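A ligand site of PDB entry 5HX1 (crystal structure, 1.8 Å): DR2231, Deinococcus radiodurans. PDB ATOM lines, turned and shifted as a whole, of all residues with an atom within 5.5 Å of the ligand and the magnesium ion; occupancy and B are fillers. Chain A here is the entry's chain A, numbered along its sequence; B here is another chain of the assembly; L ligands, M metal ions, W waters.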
ATOM      1  N   VAL A  99     -20.178 -19.977 -17.205  1.00  0.00           N
ATOM      2  CA  VAL A  99     -18.983 -19.196 -17.524  1.00  0.00           C
ATOM      3  C   VAL A  99     -17.735 -19.875 -16.965  1.00  0.00           C
ATOM      4  O   VAL A  99     -16.735 -20.042 -17.674  1.00  0.00           O
ATOM      5  CB  VAL A  99     -19.146 -17.760 -17.011  1.00  0.00           C
ATOM      6  CG1 VAL A  99     -17.835 -16.953 -17.143  1.00  0.00           C
ATOM      7  CG2 VAL A  99     -20.255 -17.054 -17.802  1.00  0.00           C
ATOM      8  N   ASN A 103     -14.272 -21.304 -18.677  1.00  0.00           N
ATOM      9  CA  ASN A 103     -12.961 -20.725 -18.409  1.00  0.00           C
ATOM     10  C   ASN A 103     -11.955 -21.796 -17.971  1.00  0.00           C
ATOM     11  O   ASN A 103     -10.772 -21.707 -18.312  1.00  0.00           O
ATOM     12  CB  ASN A 103     -13.073 -19.605 -17.371  1.00  0.00           C
ATOM     13  CG  ASN A 103     -13.656 -18.323 -17.962  1.00  0.00           C
ATOM     14  OD1 ASN A 103     -13.648 -18.151 -19.175  1.00  0.00           O
ATOM     15  ND2 ASN A 103     -14.154 -17.435 -17.116  1.00  0.00           N
ATOM     16  N   LYS A 106      -9.916 -23.300 -20.798  1.00  0.00           N
ATOM     17  CA  LYS A 106      -8.832 -22.523 -21.392  1.00  0.00           C
ATOM     18  C   LYS A 106      -7.431 -22.940 -20.933  1.00  0.00           C
ATOM     19  O   LYS A 106      -6.448 -22.411 -21.454  1.00  0.00           O
ATOM     20  CB  LYS A 106      -9.025 -21.036 -21.063  1.00  0.00           C
ATOM     21  CG  LYS A 106     -10.325 -20.470 -21.621  1.00  0.00           C
ATOM     22  CD  LYS A 106     -10.566 -19.037 -21.138  1.00  0.00           C
ATOM     23  CE  LYS A 106     -11.818 -18.491 -21.841  1.00  0.00           C
ATOM     24  NZ  LYS A 106     -12.064 -17.049 -21.565  1.00  0.00           N
ATOM     25  N   GLY A 115      -0.200 -11.411 -18.866  1.00  0.00           N
ATOM     26  CA  GLY A 115      -0.653 -12.474 -17.981  1.00  0.00           C
ATOM     27  C   GLY A 115      -2.030 -13.020 -18.328  1.00  0.00           C
ATOM     28  O   GLY A 115      -2.408 -14.068 -17.799  1.00  0.00           O
ATOM     29  N   LYS A 116      -2.780 -12.347 -19.201  1.00  0.00           N
ATOM     30  CA  LYS A 116      -4.115 -12.833 -19.512  1.00  0.00           C
ATOM     31  C   LYS A 116      -4.074 -14.221 -20.144  1.00  0.00           C
ATOM     32  O   LYS A 116      -3.328 -14.473 -21.094  1.00  0.00           O
ATOM     33  CB  LYS A 116      -4.830 -11.868 -20.468  1.00  0.00           C
ATOM     34  CG  LYS A 116      -6.243 -12.382 -20.776  1.00  0.00           C
ATOM     35  CD  LYS A 116      -6.968 -11.428 -21.716  1.00  0.00           C
ATOM     36  CE  LYS A 116      -8.416 -11.902 -21.961  1.00  0.00           C
ATOM     37  NZ  LYS A 116      -9.216 -11.007 -22.897  1.00  0.00           N
ATOM     38  N   GLN A 117      -4.900 -15.130 -19.599  1.00  0.00           N
ATOM     39  CA  GLN A 117      -5.061 -16.456 -20.190  1.00  0.00           C
ATOM     40  C   GLN A 117      -5.843 -16.383 -21.511  1.00  0.00           C
ATOM     41  O   GLN A 117      -6.932 -15.801 -21.559  1.00  0.00           O
ATOM     42  CB  GLN A 117      -5.794 -17.378 -19.210  1.00  0.00           C
ATOM     43  CG  GLN A 117      -6.032 -18.772 -19.731  1.00  0.00           C
ATOM     44  CD  GLN A 117      -4.737 -19.515 -19.977  1.00  0.00           C
ATOM     45  OE1 GLN A 117      -3.901 -19.612 -19.081  1.00  0.00           O
ATOM     46  NE2 GLN A 117      -4.546 -20.011 -21.198  1.00  0.00           N
ATOM     47  N   LEU A 118      -5.290 -16.976 -22.566  1.00  0.00           N
ATOM     48  CA  LEU A 118      -5.905 -16.965 -23.880  1.00  0.00           C
ATOM     49  C   LEU A 118      -6.501 -18.339 -24.217  1.00  0.00           C
ATOM     50  O   LEU A 118      -6.291 -19.341 -23.531  1.00  0.00           O
ATOM     51  CB  LEU A 118      -4.879 -16.534 -24.949  1.00  0.00           C
ATOM     52  CG  LEU A 118      -4.311 -15.120 -24.717  1.00  0.00           C
ATOM     53  CD1 LEU A 118      -3.309 -14.744 -25.811  1.00  0.00           C
ATOM     54  CD2 LEU A 118      -5.419 -14.058 -24.654  1.00  0.00           C
ATOM     55  N   LYS A 119      -7.272 -18.370 -25.321  1.00  0.00           N
ATOM     56  CA  LYS A 119      -8.028 -19.591 -25.589  1.00  0.00           C
ATOM     57  C   LYS A 119      -7.240 -20.535 -26.487  1.00  0.00           C
ATOM     58  O   LYS A 119      -6.624 -20.083 -27.468  1.00  0.00           O
ATOM     59  CB  LYS A 119      -9.372 -19.249 -26.259  1.00  0.00           C
ATOM     60  CG  LYS A 119     -10.298 -18.459 -25.327  1.00  0.00           C
ATOM     61  CD  LYS A 119     -11.179 -17.477 -26.110  1.00  0.00           C
ATOM     62  CE  LYS A 119     -12.032 -16.610 -25.171  1.00  0.00           C
ATOM     63  NZ  LYS A 119     -12.891 -15.606 -25.919  1.00  0.00           N
ATOM     64  N   LEU B   8     -12.902 -19.200  -8.579  1.00  0.00           N
ATOM     65  CA  LEU B   8     -11.744 -18.459  -9.089  1.00  0.00           C
ATOM     66  C   LEU B   8     -10.432 -19.095  -8.630  1.00  0.00           C
ATOM     67  O   LEU B   8      -9.453 -19.128  -9.391  1.00  0.00           O
ATOM     68  CB  LEU B   8     -11.806 -16.997  -8.669  1.00  0.00           C
ATOM     69  CG  LEU B   8     -12.286 -16.026  -9.761  1.00  0.00           C
ATOM     70  CD1 LEU B   8     -11.318 -16.049 -10.958  1.00  0.00           C
ATOM     71  CD2 LEU B   8     -13.689 -16.395 -10.239  1.00  0.00           C
ATOM     72  N   PHE B  11      -9.759 -21.954 -10.910  1.00  0.00           N
ATOM     73  CA  PHE B  11      -9.324 -21.486 -12.225  1.00  0.00           C
ATOM     74  C   PHE B  11      -7.871 -21.046 -12.182  1.00  0.00           C
ATOM     75  O   PHE B  11      -7.065 -21.412 -13.059  1.00  0.00           O
ATOM     76  CB  PHE B  11     -10.241 -20.356 -12.693  1.00  0.00           C
ATOM     77  CG  PHE B  11      -9.749 -19.623 -13.922  1.00  0.00           C
ATOM     78  CD1 PHE B  11      -9.815 -20.210 -15.182  1.00  0.00           C
ATOM     79  CD2 PHE B  11      -9.270 -18.329 -13.820  1.00  0.00           C
ATOM     80  CE1 PHE B  11      -9.373 -19.522 -16.314  1.00  0.00           C
ATOM     81  CE2 PHE B  11      -8.844 -17.630 -14.939  1.00  0.00           C
ATOM     82  CZ  PHE B  11      -8.880 -18.223 -16.194  1.00  0.00           C
ATOM     83  N   HIS B  12      -7.502 -20.253 -11.183  1.00  0.00           N
ATOM     84  CA  HIS B  12      -6.120 -19.773 -11.120  1.00  0.00           C
ATOM     85  C   HIS B  12      -5.152 -20.914 -10.864  1.00  0.00           C
ATOM     86  O   HIS B  12      -4.051 -20.914 -11.422  1.00  0.00           O
ATOM     87  CB  HIS B  12      -6.009 -18.675 -10.055  1.00  0.00           C
ATOM     88  CG  HIS B  12      -6.580 -17.364 -10.501  1.00  0.00           C
ATOM     89  ND1 HIS B  12      -7.081 -16.419  -9.621  1.00  0.00           N
ATOM     90  CD2 HIS B  12      -6.784 -16.862 -11.747  1.00  0.00           C
ATOM     91  CE1 HIS B  12      -7.540 -15.383 -10.302  1.00  0.00           C
ATOM     92  NE2 HIS B  12      -7.365 -15.621 -11.589  1.00  0.00           N
ATOM     93  N   ILE B  15      -4.651 -22.661 -14.315  1.00  0.00           N
ATOM     94  CA  ILE B  15      -3.863 -21.959 -15.330  1.00  0.00           C
ATOM     95  C   ILE B  15      -2.485 -21.528 -14.818  1.00  0.00           C
ATOM     96  O   ILE B  15      -1.725 -20.888 -15.566  1.00  0.00           O
ATOM     97  CB  ILE B  15      -4.625 -20.734 -15.871  1.00  0.00           C
ATOM     98  CG1 ILE B  15      -4.759 -19.657 -14.790  1.00  0.00           C
ATOM     99  CG2 ILE B  15      -6.015 -21.157 -16.356  1.00  0.00           C
ATOM    100  CD1 ILE B  15      -5.227 -18.308 -15.349  1.00  0.00           C
ATOM    101  N   LEU B  33      -2.657  -5.924 -14.771  1.00  0.00           N
ATOM    102  CA  LEU B  33      -3.504  -6.924 -15.420  1.00  0.00           C
ATOM    103  C   LEU B  33      -4.935  -6.839 -14.898  1.00  0.00           C
ATOM    104  O   LEU B  33      -5.886  -6.889 -15.690  1.00  0.00           O
ATOM    105  CB  LEU B  33      -2.953  -8.334 -15.203  1.00  0.00           C
ATOM    106  CG  LEU B  33      -3.905  -9.450 -15.686  1.00  0.00           C
ATOM    107  CD1 LEU B  33      -4.043  -9.373 -17.219  1.00  0.00           C
ATOM    108  CD2 LEU B  33      -3.401 -10.829 -15.255  1.00  0.00           C
ATOM    109  N   ARG B  34      -5.104  -6.740 -13.578  1.00  0.00           N
ATOM    110  CA  ARG B  34      -6.468  -6.711 -13.035  1.00  0.00           C
ATOM    111  C   ARG B  34      -7.221  -5.504 -13.537  1.00  0.00           C
ATOM    112  O   ARG B  34      -8.427  -5.578 -13.808  1.00  0.00           O
ATOM    113  CB  ARG B  34      -6.464  -6.724 -11.502  1.00  0.00           C
ATOM    114  CG  ARG B  34      -5.738  -7.892 -10.798  1.00  0.00           C
ATOM    115  CD  ARG B  34      -5.946  -9.272 -11.460  1.00  0.00           C
ATOM    116  NE  ARG B  34      -7.335  -9.659 -11.751  1.00  0.00           N
ATOM    117  CZ  ARG B  34      -7.673 -10.848 -12.295  1.00  0.00           C
ATOM    118  NH1 ARG B  34      -6.731 -11.738 -12.575  1.00  0.00           N
ATOM    119  NH2 ARG B  34      -8.945 -11.136 -12.564  1.00  0.00           N
ATOM    120  N   LEU B  37      -8.329  -6.187 -17.181  1.00  0.00           N
ATOM    121  CA  LEU B  37      -9.444  -7.129 -17.291  1.00  0.00           C
ATOM    122  C   LEU B  37     -10.741  -6.509 -16.813  1.00  0.00           C
ATOM    123  O   LEU B  37     -11.797  -6.729 -17.418  1.00  0.00           O
ATOM    124  CB  LEU B  37      -9.152  -8.403 -16.515  1.00  0.00           C
ATOM    125  CG  LEU B  37      -7.915  -9.179 -16.974  1.00  0.00           C
ATOM    126  CD1 LEU B  37      -7.830 -10.436 -16.127  1.00  0.00           C
ATOM    127  CD2 LEU B  37      -8.037  -9.510 -18.469  1.00  0.00           C
ATOM    128  N   GLU B  41     -14.191  -5.896 -19.184  1.00  0.00           N
ATOM    129  CA  GLU B  41     -15.524  -6.438 -18.929  1.00  0.00           C
ATOM    130  C   GLU B  41     -16.536  -5.337 -18.677  1.00  0.00           C
ATOM    131  O   GLU B  41     -17.694  -5.459 -19.107  1.00  0.00           O
ATOM    132  CB  GLU B  41     -15.498  -7.451 -17.763  1.00  0.00           C
ATOM    133  CG  GLU B  41     -14.664  -8.734 -18.026  1.00  0.00           C
ATOM    134  CD  GLU B  41     -14.828  -9.366 -19.431  1.00  0.00           C
ATOM    135  OE1 GLU B  41     -15.906  -9.283 -20.048  1.00  0.00           O
ATOM    136  OE2 GLU B  41     -13.854  -9.989 -19.911  1.00  0.00           O
ATOM    137  N   GLU B  44     -17.748  -4.148 -21.999  1.00  0.00           N
ATOM    138  CA  GLU B  44     -18.640  -5.096 -22.670  1.00  0.00           C
ATOM    139  C   GLU B  44     -20.025  -5.074 -22.047  1.00  0.00           C
ATOM    140  O   GLU B  44     -21.034  -5.167 -22.747  1.00  0.00           O
ATOM    141  CB  GLU B  44     -18.059  -6.499 -22.619  1.00  0.00           C
ATOM    142  CG  GLU B  44     -16.817  -6.690 -23.472  1.00  0.00           C
ATOM    143  CD  GLU B  44     -17.053  -6.271 -24.897  1.00  0.00           C
ATOM    144  OE1 GLU B  44     -18.068  -6.694 -25.500  1.00  0.00           O
ATOM    145  OE2 GLU B  44     -16.225  -5.499 -25.423  1.00  0.00           O
ATOM    146  N   GLU B  73     -21.942 -11.049 -19.943  1.00  0.00           N
ATOM    147  CA  GLU B  73     -20.910 -10.058 -19.627  1.00  0.00           C
ATOM    148  C   GLU B  73     -20.912  -9.703 -18.151  1.00  0.00           C
ATOM    149  O   GLU B  73     -19.846  -9.482 -17.563  1.00  0.00           O
ATOM    150  CB  GLU B  73     -21.075  -8.813 -20.506  1.00  0.00           C
ATOM    151  CG  GLU B  73     -20.973  -9.066 -22.037  1.00  0.00           C
ATOM    152  CD  GLU B  73     -19.653  -9.684 -22.491  1.00  0.00           C
ATOM    153  OE1 GLU B  73     -18.663  -9.646 -21.735  1.00  0.00           O
ATOM    154  OE2 GLU B  73     -19.614 -10.213 -23.636  1.00  0.00           O
ATOM    155  N   ALA B  75     -21.611 -11.811 -15.794  1.00  0.00           N
ATOM    156  CA  ALA B  75     -20.879 -12.927 -15.186  1.00  0.00           C
ATOM    157  C   ALA B  75     -19.364 -12.810 -15.417  1.00  0.00           C
ATOM    158  O   ALA B  75     -18.569 -13.134 -14.529  1.00  0.00           O
ATOM    159  CB  ALA B  75     -21.408 -14.247 -15.712  1.00  0.00           C
ATOM    160  N   ASP B  76     -18.949 -12.374 -16.619  1.00  0.00           N
ATOM    161  CA  ASP B  76     -17.534 -12.103 -16.874  1.00  0.00           C
ATOM    162  C   ASP B  76     -16.993 -11.048 -15.922  1.00  0.00           C
ATOM    163  O   ASP B  76     -15.865 -11.165 -15.416  1.00  0.00           O
ATOM    164  CB  ASP B  76     -17.327 -11.599 -18.309  1.00  0.00           C
ATOM    165  CG  ASP B  76     -17.281 -12.707 -19.348  1.00  0.00           C
ATOM    166  OD1 ASP B  76     -17.247 -13.902 -18.968  1.00  0.00           O
ATOM    167  OD2 ASP B  76     -17.271 -12.350 -20.565  1.00  0.00           O
ATOM    168  N   TYR B  79     -16.491 -12.473 -12.704  1.00  0.00           N
ATOM    169  CA  TYR B  79     -15.342 -13.359 -12.761  1.00  0.00           C
ATOM    170  C   TYR B  79     -14.034 -12.605 -12.579  1.00  0.00           C
ATOM    171  O   TYR B  79     -13.155 -13.050 -11.821  1.00  0.00           O
ATOM    172  CB  TYR B  79     -15.344 -14.122 -14.095  1.00  0.00           C
ATOM    173  CG  TYR B  79     -14.746 -15.504 -14.000  1.00  0.00           C
ATOM    174  CD1 TYR B  79     -15.538 -16.594 -13.671  1.00  0.00           C
ATOM    175  CD2 TYR B  79     -13.368 -15.713 -14.215  1.00  0.00           C
ATOM    176  CE1 TYR B  79     -15.006 -17.862 -13.572  1.00  0.00           C
ATOM    177  CE2 TYR B  79     -12.825 -16.973 -14.110  1.00  0.00           C
ATOM    178  CZ  TYR B  79     -13.633 -18.049 -13.789  1.00  0.00           C
ATOM    179  OH  TYR B  79     -13.117 -19.305 -13.675  1.00  0.00           O
ATOM    180  N   VAL B  80     -13.872 -11.448 -13.241  1.00  0.00           N
ATOM    181  CA  VAL B  80     -12.613 -10.716 -13.131  1.00  0.00           C
ATOM    182  C   VAL B  80     -12.561  -9.882 -11.858  1.00  0.00           C
ATOM    183  O   VAL B  80     -11.474  -9.456 -11.455  1.00  0.00           O
ATOM    184  CB  VAL B  80     -12.348  -9.829 -14.362  1.00  0.00           C
ATOM    185  CG1 VAL B  80     -12.315 -10.677 -15.647  1.00  0.00           C
ATOM    186  CG2 VAL B  80     -13.393  -8.710 -14.502  1.00  0.00           C
HETATM  187  N1  LIG L   1     -10.575 -14.658 -17.719  1.00  0.00           N
HETATM  188  C1  LIG L   1      -9.898 -14.506 -16.400  1.00  0.00           C
HETATM  189  N2  LIG L   1      -8.412 -14.359 -16.362  1.00  0.00           N
HETATM  190  C2  LIG L   1      -7.637 -14.365 -17.582  1.00  0.00           C
HETATM  191  C3  LIG L   1      -8.323 -14.517 -18.883  1.00  0.00           C
HETATM  192  C4  LIG L   1      -9.806 -14.674 -18.931  1.00  0.00           C
HETATM  193  O1  LIG L   1     -10.517 -14.500 -15.392  1.00  0.00           O
HETATM  194  O2  LIG L   1      -6.455 -14.237 -17.525  1.00  0.00           O
HETATM  195  C5  LIG L   1     -12.031 -14.847 -17.789  1.00  0.00           C
HETATM  196  C6  LIG L   1     -12.832 -13.509 -17.518  1.00  0.00           C
HETATM  197  C7  LIG L   1     -14.041 -13.713 -18.420  1.00  0.00           C
HETATM  198  C8  LIG L   1     -13.531 -14.300 -19.542  1.00  0.00           C
HETATM  199  O3  LIG L   1     -14.991 -14.649 -17.738  1.00  0.00           O
HETATM  200  O4  LIG L   1     -12.336 -15.243 -19.009  1.00  0.00           O
HETATM  201  C9  LIG L   1     -12.954 -13.308 -20.523  1.00  0.00           C
HETATM  202  O5  LIG L   1     -12.072 -13.959 -21.439  1.00  0.00           O
HETATM  203  P1  LIG L   1     -12.002 -13.414 -22.990  1.00  0.00           P
HETATM  204  O6  LIG L   1     -13.313 -13.786 -23.647  1.00  0.00           O
HETATM  205  O7  LIG L   1     -10.843 -14.082 -23.691  1.00  0.00           O
HETATM  206  O8  LIG L   1     -11.805 -11.904 -22.974  1.00  0.00           O
HETATM  207 MG    MG M   1     -16.554 -10.477 -21.811  1.00  0.00          MG
HETATM  208  O   HOH W   1      -9.598 -15.882 -22.337  1.00  0.00           O
HETATM  209  O   HOH W   2     -15.189 -12.619 -25.158  1.00  0.00           O
HETATM  210  O   HOH W   3     -13.801 -10.328 -22.492  1.00  0.00           O
HETATM  211  O   HOH W   4     -14.171 -16.174 -22.575  1.00  0.00           O
HETATM  212  O   HOH W   5      -4.605 -14.685 -15.377  1.00  0.00           O
HETATM  213  O   HOH W   6     -16.473 -10.860 -23.563  1.00  0.00           O
HETATM  214  O   HOH W   7     -16.126 -13.349 -23.055  1.00  0.00           O
HETATM  215  O   HOH W   8      -6.962 -14.144 -14.039  1.00  0.00           O
HETATM  216  O   HOH W   9      -9.852 -13.610 -13.143  1.00  0.00           O
HETATM  217  O   HOH W  10      -9.458 -13.869 -25.904  1.00  0.00           O
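CG1 of Val 99 touches O3 of the ligand (3.7 Å). Phe 11 of chain B touches the ligand (CE2 to O1, 3.6 Å). Leu 37 of chain B touches the ligand. CD2 of Tyr 79 of chain B touches O1 of the ligand (3.3 Å). Val 80 of chain B touches the ligand. Of the 22 residues printed, 12 come within 4 Å of the ligand. The nearest printed residue that does not touch the ligand is Gly 115 (4.1 Å).
Water W3 lies within hydrogen-bond range of O8 of the ligand (2.6 Å) and OE2 of Glu 41 of chain B (2.6 Å). Water W9 lies within hydrogen-bond range of O1 of the ligand (2.5 Å) and NH2 of Arg 34 of chain B (2.7 Å). Water W1 lies within hydrogen-bond range of an oxygen (O7) of the ligand, the backbone carbonyl oxygen (O) of Gln 117 and the side-chain amino group (NZ) of Lys 106. Water W8 lies within hydrogen-bond range of N2 of the ligand (2.7 Å), NH1 of Arg 34 of chain B (2.8 Å) and NE2 of His 12 of chain B (2.9 Å). Water W4 lies within hydrogen-bond range of NZ of Lys 106 (2.5 Å) and O6 of the ligand (2.8 Å). Water W5 bridges O2 of the ligand and O of Gly 115.
An oxygen (O3) of the ligand sits at hydrogen-bond distance from the side-chain amide nitrogen (ND2) of Asn 103, at 3.0 Å. O3 of the ligand lies within hydrogen-bond range of OD1 of Asp 76 of chain B (2.7 Å). The side-chain amino group (NZ) of Lys 116 is in salt-bridge range of an oxygen (O8) of the ligand, at 2.7 Å. NZ of Lys 106 lies within salt-bridge range of O7 of the ligand, at 3.8 Å. O2 of the ligand lies within hydrogen-bond range of N of Gln 117 (2.7 Å). The side-chain amino group of Lys 119 is in salt-bridge range of an oxygen (O6) of the ligand (2.9 Å).
The magnesium ion is bound by water W6, OE1 of Glu 41 of chain B, OE1 of Glu 73 of chain B and OD2 of Asp 76 of chain B. The magnesium ion has four donor atoms within binding distance. Slightly farther from the magnesium ion lies water W3 (2.8 Å).
The side-chain amide oxygen (OD1) of Asn 103 is in hydrogen-bond range of the side-chain amino group (NZ) of Lys 106 (3.1 Å). The guanidinium group (NH2) of Arg 34 of chain B lies within hydrogen-bond range of the backbone carbonyl oxygen (O) of Val 80 of chain B, 3.2 Å away. O of Lys 106 lies within hydrogen-bond range of NE2 of Gln 117, at 3.1 Å.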
